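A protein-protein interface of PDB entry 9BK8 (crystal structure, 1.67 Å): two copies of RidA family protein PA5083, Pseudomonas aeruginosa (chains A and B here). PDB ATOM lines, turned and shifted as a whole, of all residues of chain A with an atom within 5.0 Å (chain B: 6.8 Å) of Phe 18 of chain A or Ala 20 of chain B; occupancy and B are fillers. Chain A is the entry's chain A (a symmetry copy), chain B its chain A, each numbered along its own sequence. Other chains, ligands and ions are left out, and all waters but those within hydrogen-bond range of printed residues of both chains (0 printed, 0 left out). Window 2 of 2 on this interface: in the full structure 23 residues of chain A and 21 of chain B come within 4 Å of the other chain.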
ATOM      1  N   MET A   1     -19.006  -5.997 -19.417  1.00  0.00           N
ATOM      2  CA  MET A   1     -19.860  -5.099 -20.229  1.00  0.00           C
ATOM      3  C   MET A   1     -19.881  -3.677 -19.690  1.00  0.00           C
ATOM      4  O   MET A   1     -20.460  -2.797 -20.322  1.00  0.00           O
ATOM      5  CB  MET A   1     -21.293  -5.635 -20.287  1.00  0.00           C
ATOM      6  CG  MET A   1     -22.089  -5.414 -19.006  1.00  0.00           C
ATOM      7  SD  MET A   1     -23.164  -3.960 -19.043  1.00  0.00           S
ATOM      8  CE  MET A   1     -24.189  -4.336 -20.464  1.00  0.00           C
ATOM      9  N   GLU A   2     -19.274  -3.451 -18.525  1.00  0.00           N
ATOM     10  CA  GLU A   2     -19.176  -2.109 -17.968  1.00  0.00           C
ATOM     11  C   GLU A   2     -17.719  -1.727 -17.775  1.00  0.00           C
ATOM     12  O   GLU A   2     -16.944  -2.516 -17.215  1.00  0.00           O
ATOM     13  CB  GLU A   2     -19.920  -2.001 -16.617  1.00  0.00           C
ATOM     14  CG  GLU A   2     -21.131  -1.075 -16.652  1.00  0.00           C
ATOM     15  CD  GLU A   2     -21.775  -0.886 -15.289  1.00  0.00           C
ATOM     16  OE1 GLU A   2     -23.022  -0.785 -15.222  1.00  0.00           O
ATOM     17  OE2 GLU A   2     -21.032  -0.846 -14.285  1.00  0.00           O
ATOM     18  N   PRO A   3     -17.296  -0.538 -18.197  1.00  0.00           N
ATOM     19  CA  PRO A   3     -15.972  -0.049 -17.793  1.00  0.00           C
ATOM     20  C   PRO A   3     -15.853   0.073 -16.277  1.00  0.00           C
ATOM     21  O   PRO A   3     -16.809   0.437 -15.586  1.00  0.00           O
ATOM     22  CB  PRO A   3     -15.874   1.329 -18.452  1.00  0.00           C
ATOM     23  CG  PRO A   3     -16.981   1.419 -19.411  1.00  0.00           C
ATOM     24  CD  PRO A   3     -18.036   0.442 -19.009  1.00  0.00           C
ATOM     25  N   VAL A  16      -8.823   3.272 -16.961  1.00  0.00           N
ATOM     26  CA  VAL A  16     -10.142   2.719 -17.256  1.00  0.00           C
ATOM     27  C   VAL A  16      -9.951   1.344 -17.872  1.00  0.00           C
ATOM     28  O   VAL A  16      -9.230   1.188 -18.861  1.00  0.00           O
ATOM     29  CB  VAL A  16     -10.962   3.624 -18.184  1.00  0.00           C
ATOM     30  CG1 VAL A  16     -12.267   2.946 -18.519  1.00  0.00           C
ATOM     31  CG2 VAL A  16     -11.222   4.965 -17.525  1.00  0.00           C
ATOM     32  N   CYS A  17     -10.599   0.342 -17.290  1.00  0.00           N
ATOM     33  CA  CYS A  17     -10.557  -1.013 -17.810  1.00  0.00           C
ATOM     34  C   CYS A  17     -11.873  -1.355 -18.490  1.00  0.00           C
ATOM     35  O   CYS A  17     -12.954  -1.008 -18.000  1.00  0.00           O
ATOM     36  CB  CYS A  17     -10.281  -2.013 -16.688  1.00  0.00           C
ATOM     37  SG  CYS A  17      -8.776  -1.617 -15.759  1.00  0.00           S
ATOM     38  N   PHE A  18     -11.772  -2.019 -19.634  1.00  0.00           N
ATOM     39  CA  PHE A  18     -12.961  -2.488 -20.342  1.00  0.00           C
ATOM     40  C   PHE A  18     -12.624  -3.807 -21.014  1.00  0.00           C
ATOM     41  O   PHE A  18     -11.778  -3.858 -21.910  1.00  0.00           O
ATOM     42  CB  PHE A  18     -13.474  -1.454 -21.349  1.00  0.00           C
ATOM     43  CG  PHE A  18     -14.706  -1.913 -22.075  1.00  0.00           C
ATOM     44  CD1 PHE A  18     -15.875  -2.148 -21.380  1.00  0.00           C
ATOM     45  CD2 PHE A  18     -14.677  -2.158 -23.425  1.00  0.00           C
ATOM     46  CE1 PHE A  18     -16.996  -2.610 -22.027  1.00  0.00           C
ATOM     47  CE2 PHE A  18     -15.799  -2.623 -24.085  1.00  0.00           C
ATOM     48  CZ  PHE A  18     -16.956  -2.853 -23.378  1.00  0.00           C
ATOM     49  N   ASP A  19     -13.281  -4.887 -20.558  1.00  0.00           N
ATOM     50  CA  ASP A  19     -12.969  -6.239 -21.001  1.00  0.00           C
ATOM     51  C   ASP A  19     -11.482  -6.499 -20.815  1.00  0.00           C
ATOM     52  O   ASP A  19     -10.978  -6.402 -19.696  1.00  0.00           O
ATOM     53  CB  ASP A  19     -13.392  -6.455 -22.454  1.00  0.00           C
ATOM     54  CG  ASP A  19     -13.673  -7.923 -22.772  1.00  0.00           C
ATOM     55  OD1 ASP A  19     -13.473  -8.799 -21.894  1.00  0.00           O
ATOM     56  OD2 ASP A  19     -14.077  -8.200 -23.916  1.00  0.00           O
ATOM     57  N   ALA A  20     -10.767  -6.829 -21.887  1.00  0.00           N
ATOM     58  CA  ALA A  20      -9.357  -7.171 -21.785  1.00  0.00           C
ATOM     59  C   ALA A  20      -8.444  -5.987 -22.045  1.00  0.00           C
ATOM     60  O   ALA A  20      -7.237  -6.184 -22.221  1.00  0.00           O
ATOM     61  CB  ALA A  20      -9.000  -8.296 -22.754  1.00  0.00           C
ATOM     62  N   LEU A  21      -8.984  -4.777 -22.090  1.00  0.00           N
ATOM     63  CA  LEU A  21      -8.183  -3.595 -22.395  1.00  0.00           C
ATOM     64  C   LEU A  21      -8.066  -2.682 -21.181  1.00  0.00           C
ATOM     65  O   LEU A  21      -8.985  -2.570 -20.367  1.00  0.00           O
ATOM     66  CB  LEU A  21      -8.795  -2.825 -23.574  1.00  0.00           C
ATOM     67  CG  LEU A  21      -8.720  -3.542 -24.929  1.00  0.00           C
ATOM     68  CD1 LEU A  21      -9.494  -2.696 -25.975  1.00  0.00           C
ATOM     69  CD2 LEU A  21      -7.318  -3.791 -25.379  1.00  0.00           C
ATOM     70  N   PHE A  23      -6.865   1.329 -20.449  1.00  0.00           N
ATOM     71  CA  PHE A  23      -6.551   2.656 -20.980  1.00  0.00           C
ATOM     72  C   PHE A  23      -6.019   3.509 -19.834  1.00  0.00           C
ATOM     73  O   PHE A  23      -6.743   3.782 -18.875  1.00  0.00           O
ATOM     74  CB  PHE A  23      -7.793   3.323 -21.589  1.00  0.00           C
ATOM     75  CG  PHE A  23      -8.411   2.556 -22.722  1.00  0.00           C
ATOM     76  CD1 PHE A  23      -9.228   1.459 -22.482  1.00  0.00           C
ATOM     77  CD2 PHE A  23      -8.184   2.938 -24.024  1.00  0.00           C
ATOM     78  CE1 PHE A  23      -9.782   0.741 -23.543  1.00  0.00           C
ATOM     79  CE2 PHE A  23      -8.746   2.230 -25.079  1.00  0.00           C
ATOM     80  CZ  PHE A  23      -9.535   1.131 -24.835  1.00  0.00           C
ATOM     81  N   ARG A 115      -5.135  -6.563 -20.470  1.00  0.00           N
ATOM     82  CA  ARG A 115      -5.265  -7.198 -19.166  1.00  0.00           C
ATOM     83  C   ARG A 115      -4.820  -8.647 -19.264  1.00  0.00           C
ATOM     84  O   ARG A 115      -4.949  -9.288 -20.311  1.00  0.00           O
ATOM     85  CB  ARG A 115      -6.706  -7.123 -18.653  1.00  0.00           C
ATOM     86  CG  ARG A 115      -7.067  -5.754 -18.104  1.00  0.00           C
ATOM     87  CD  ARG A 115      -8.095  -5.798 -16.970  1.00  0.00           C
ATOM     88  NE  ARG A 115      -9.476  -5.804 -17.447  1.00  0.00           N
ATOM     89  CZ  ARG A 115     -10.538  -5.594 -16.677  1.00  0.00           C
ATOM     90  NH1 ARG A 115     -10.416  -5.359 -15.378  1.00  0.00           N
ATOM     91  NH2 ARG A 115     -11.755  -5.600 -17.228  1.00  0.00           N
ATOM     92  N   CYS B  17     -17.431   1.916 -35.517  1.00  0.00           N
ATOM     93  CA  CYS B  17     -17.730   0.930 -34.496  1.00  0.00           C
ATOM     94  C   CYS B  17     -17.139  -0.419 -34.877  1.00  0.00           C
ATOM     95  O   CYS B  17     -17.187  -0.830 -36.042  1.00  0.00           O
ATOM     96  CB  CYS B  17     -19.241   0.794 -34.302  1.00  0.00           C
ATOM     97  SG  CYS B  17     -20.040   2.380 -33.942  1.00  0.00           S
ATOM     98  N   PHE B  18     -16.561  -1.090 -33.890  1.00  0.00           N
ATOM     99  CA  PHE B  18     -16.034  -2.437 -34.103  1.00  0.00           C
ATOM    100  C   PHE B  18     -16.235  -3.232 -32.825  1.00  0.00           C
ATOM    101  O   PHE B  18     -15.654  -2.910 -31.786  1.00  0.00           O
ATOM    102  CB  PHE B  18     -14.564  -2.417 -34.531  1.00  0.00           C
ATOM    103  CG  PHE B  18     -14.010  -3.793 -34.770  1.00  0.00           C
ATOM    104  CD1 PHE B  18     -14.526  -4.584 -35.775  1.00  0.00           C
ATOM    105  CD2 PHE B  18     -13.025  -4.305 -33.962  1.00  0.00           C
ATOM    106  CE1 PHE B  18     -14.057  -5.861 -35.974  1.00  0.00           C
ATOM    107  CE2 PHE B  18     -12.546  -5.587 -34.154  1.00  0.00           C
ATOM    108  CZ  PHE B  18     -13.072  -6.364 -35.160  1.00  0.00           C
ATOM    109  N   ASP B  19     -17.086  -4.270 -32.902  1.00  0.00           N
ATOM    110  CA  ASP B  19     -17.491  -5.040 -31.735  1.00  0.00           C
ATOM    111  C   ASP B  19     -18.022  -4.095 -30.667  1.00  0.00           C
ATOM    112  O   ASP B  19     -18.979  -3.363 -30.918  1.00  0.00           O
ATOM    113  CB  ASP B  19     -16.334  -5.884 -31.202  1.00  0.00           C
ATOM    114  CG  ASP B  19     -16.810  -7.118 -30.435  1.00  0.00           C
ATOM    115  OD1 ASP B  19     -18.039  -7.295 -30.244  1.00  0.00           O
ATOM    116  OD2 ASP B  19     -15.943  -7.902 -30.006  1.00  0.00           O
ATOM    117  N   ALA B  20     -17.423  -4.095 -29.480  1.00  0.00           N
ATOM    118  CA  ALA B  20     -17.915  -3.281 -28.379  1.00  0.00           C
ATOM    119  C   ALA B  20     -17.213  -1.940 -28.279  1.00  0.00           C
ATOM    120  O   ALA B  20     -17.365  -1.254 -27.262  1.00  0.00           O
ATOM    121  CB  ALA B  20     -17.769  -4.020 -27.052  1.00  0.00           C
ATOM    122  N   LEU B  21     -16.441  -1.559 -29.289  1.00  0.00           N
ATOM    123  CA  LEU B  21     -15.685  -0.311 -29.241  1.00  0.00           C
ATOM    124  C   LEU B  21     -16.223   0.697 -30.250  1.00  0.00           C
ATOM    125  O   LEU B  21     -16.692   0.340 -31.331  1.00  0.00           O
ATOM    126  CB  LEU B  21     -14.197  -0.580 -29.511  1.00  0.00           C
ATOM    127  CG  LEU B  21     -13.467  -1.363 -28.411  1.00  0.00           C
ATOM    128  CD1 LEU B  21     -12.024  -1.661 -28.896  1.00  0.00           C
ATOM    129  CD2 LEU B  21     -13.451  -0.648 -27.101  1.00  0.00           C
ATOM    130  N   VAL B  22     -16.139   1.973 -29.871  1.00  0.00           N
ATOM    131  CA  VAL B  22     -16.535   3.107 -30.689  1.00  0.00           C
ATOM    132  C   VAL B  22     -15.333   4.043 -30.768  1.00  0.00           C
ATOM    133  O   VAL B  22     -14.846   4.496 -29.731  1.00  0.00           O
ATOM    134  CB  VAL B  22     -17.740   3.855 -30.089  1.00  0.00           C
ATOM    135  CG1 VAL B  22     -18.053   5.054 -30.931  1.00  0.00           C
ATOM    136  CG2 VAL B  22     -18.946   2.912 -29.950  1.00  0.00           C
ATOM    137  N   ARG B  59     -19.675   5.798 -20.688  1.00  0.00           N
ATOM    138  CA  ARG B  59     -18.934   4.673 -21.240  1.00  0.00           C
ATOM    139  C   ARG B  59     -17.715   5.127 -22.038  1.00  0.00           C
ATOM    140  O   ARG B  59     -17.136   4.346 -22.784  1.00  0.00           O
ATOM    141  CB  ARG B  59     -19.865   3.803 -22.086  1.00  0.00           C
ATOM    142  CG  ARG B  59     -20.933   3.104 -21.222  1.00  0.00           C
ATOM    143  CD  ARG B  59     -21.860   2.194 -22.009  1.00  0.00           C
ATOM    144  NE  ARG B  59     -21.233   0.952 -22.434  1.00  0.00           N
ATOM    145  CZ  ARG B  59     -21.122  -0.138 -21.681  1.00  0.00           C
ATOM    146  NH1 ARG B  59     -21.499  -0.146 -20.415  1.00  0.00           N
ATOM    147  NH2 ARG B  59     -20.612  -1.242 -22.214  1.00  0.00           N
ATOM    148  N   LEU B  61     -13.962   5.629 -22.683  1.00  0.00           N
ATOM    149  CA  LEU B  61     -12.789   4.905 -22.226  1.00  0.00           C
ATOM    150  C   LEU B  61     -11.565   5.804 -22.189  1.00  0.00           C
ATOM    151  O   LEU B  61     -10.786   5.771 -21.215  1.00  0.00           O
ATOM    152  CB  LEU B  61     -12.543   3.708 -23.144  1.00  0.00           C
ATOM    153  CG  LEU B  61     -13.708   2.696 -23.228  1.00  0.00           C
ATOM    154  CD1 LEU B  61     -13.389   1.636 -24.248  1.00  0.00           C
ATOM    155  CD2 LEU B  61     -14.018   2.097 -21.881  1.00  0.00           C
ATOM    156  N   ALA B 113     -14.785   4.936 -26.902  1.00  0.00           N
ATOM    157  CA  ALA B 113     -15.794   4.590 -25.911  1.00  0.00           C
ATOM    158  C   ALA B 113     -16.262   3.150 -26.082  1.00  0.00           C
ATOM    159  O   ALA B 113     -16.028   2.513 -27.105  1.00  0.00           O
ATOM    160  CB  ALA B 113     -17.010   5.519 -26.006  1.00  0.00           C
ATOM    161  N   ALA B 114     -16.975   2.661 -25.079  1.00  0.00           N
ATOM    162  CA  ALA B 114     -17.536   1.312 -25.099  1.00  0.00           C
ATOM    163  C   ALA B 114     -18.999   1.346 -25.524  1.00  0.00           C
ATOM    164  O   ALA B 114     -19.791   2.122 -24.980  1.00  0.00           O
ATOM    165  CB  ALA B 114     -17.423   0.651 -23.726  1.00  0.00           C
ATOM    166  N   ARG B 115     -19.356   0.487 -26.468  1.00  0.00           N
ATOM    167  CA  ARG B 115     -20.757   0.347 -26.840  1.00  0.00           C
ATOM    168  C   ARG B 115     -21.521  -0.295 -25.695  1.00  0.00           C
ATOM    169  O   ARG B 115     -20.973  -1.091 -24.925  1.00  0.00           O
ATOM    170  CB  ARG B 115     -20.913  -0.490 -28.113  1.00  0.00           C
ATOM    171  CG  ARG B 115     -20.577   0.285 -29.375  1.00  0.00           C
ATOM    172  CD  ARG B 115     -21.378  -0.161 -30.601  1.00  0.00           C
ATOM    173  NE  ARG B 115     -20.766  -1.282 -31.309  1.00  0.00           N
ATOM    174  CZ  ARG B 115     -21.122  -1.692 -32.523  1.00  0.00           C
ATOM    175  NH1 ARG B 115     -22.094  -1.093 -33.195  1.00  0.00           N
ATOM    176  NH2 ARG B 115     -20.475  -2.715 -33.083  1.00  0.00           N
ATOM    177  N   GLY B 116     -22.793   0.075 -25.576  1.00  0.00           N
ATOM    178  CA  GLY B 116     -23.651  -0.450 -24.531  1.00  0.00           C
ATOM    179  C   GLY B 116     -24.434  -1.665 -24.988  1.00  0.00           C
ATOM    180  O   GLY B 116     -24.253  -2.133 -26.112  1.00  0.00           O
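Among the printed residues, pairs that only touch across the chains: Glu 2 of chain A with Arg 59 of chain B, Pro 3 of chain A with Arg 59 of chain B, Pro 3 of chain A with Leu 61 of chain B, Val 16 of chain A with Leu 61 of chain B, Phe 18 of chain A with Ala 20 of chain B, Phe 18 of chain A with Arg 59 of chain B, Phe 18 of chain A with Leu 61 of chain B, Phe 18 of chain A with Ala 114 of chain B and Phe 23 of chain A with Leu 61 of chain B.
The backbone carbonyl oxygen (O) of Ala 20 of chain B sits at hydrogen-bond distance from the backbone NH (N) of Arg 115 of chain B (2.8 Å). N of Ala 114 of chain B lies within hydrogen-bond range of O of Arg 59 of chain B (2.9 Å). The guanidinium group (NH2) of Arg 59 of chain B lies within hydrogen-bond range of the backbone carbonyl oxygen (O) of Arg 115 of chain B, 2.7 Å away. The backbone carbonyl oxygen (O) of Val 16 of chain A lies within hydrogen-bond range of the backbone NH (N) of Phe 23 of chain A (2.9 Å).
The backbone carbonyl oxygen (O) of Met 1 of chain A is in hydrogen-bond range of the guanidinium group (NH2) of Arg 59 of chain B (2.5 Å).
Printed residues of chain B that touch a printed residue of chain A: Ala 20, Arg 59, Leu 61 and Ala 114. Hydrophobic or aromatic side chains of chain B within 4 Å of the printed part of chain A: Ala 20, Leu 61 and Ala 114. Printed residues of chain A that touch a printed residue of chain B: Met 1, Glu 2, Pro 3, Val 16, Phe 18 and Phe 23. Along chain A the printed residues that touch a printed residue of chain B span positions 1 to 23.
Printed residues of chain B within 4 Å of Glu 2 of chain A: Arg 59 (3.9 Å). Of the printed residues of chain B, Val 16 of chain A touches Leu 61 (3.7 Å). Phe 18 of chain A touches just these residues of chain B: Ala 20 (3.8 Å), Arg 59 (3.9 Å), Leu 61 (3.6 Å) and Ala 114 (3.6 Å). Printed residues of chain B within 4 Å of Phe 23 of chain A: Leu 61. Ala 20 of chain B touches just one residue of chain A: Phe 18. Of the printed residues of chain A, Arg 59 of chain B touches Met 1, Glu 2, Pro 3 and Phe 18. Printed residues of chain A within 4 Å of Ala 114 of chain B: Phe 18. The nearest printed residue of chain A that does not touch Ala 20 of chain B is Asp 19 of chain A (6.4 Å).
Phe 18 of chain A touches Ala 20 of chain B, but with the chains exchanged Ala 20 of chain A does not touch Phe 18 of chain B (11.7 Å). 6 positions are printed for both chains. Of the 10 pairs that touch across the chains among the printed residues, none has its exchanged pair printed and touching as well.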
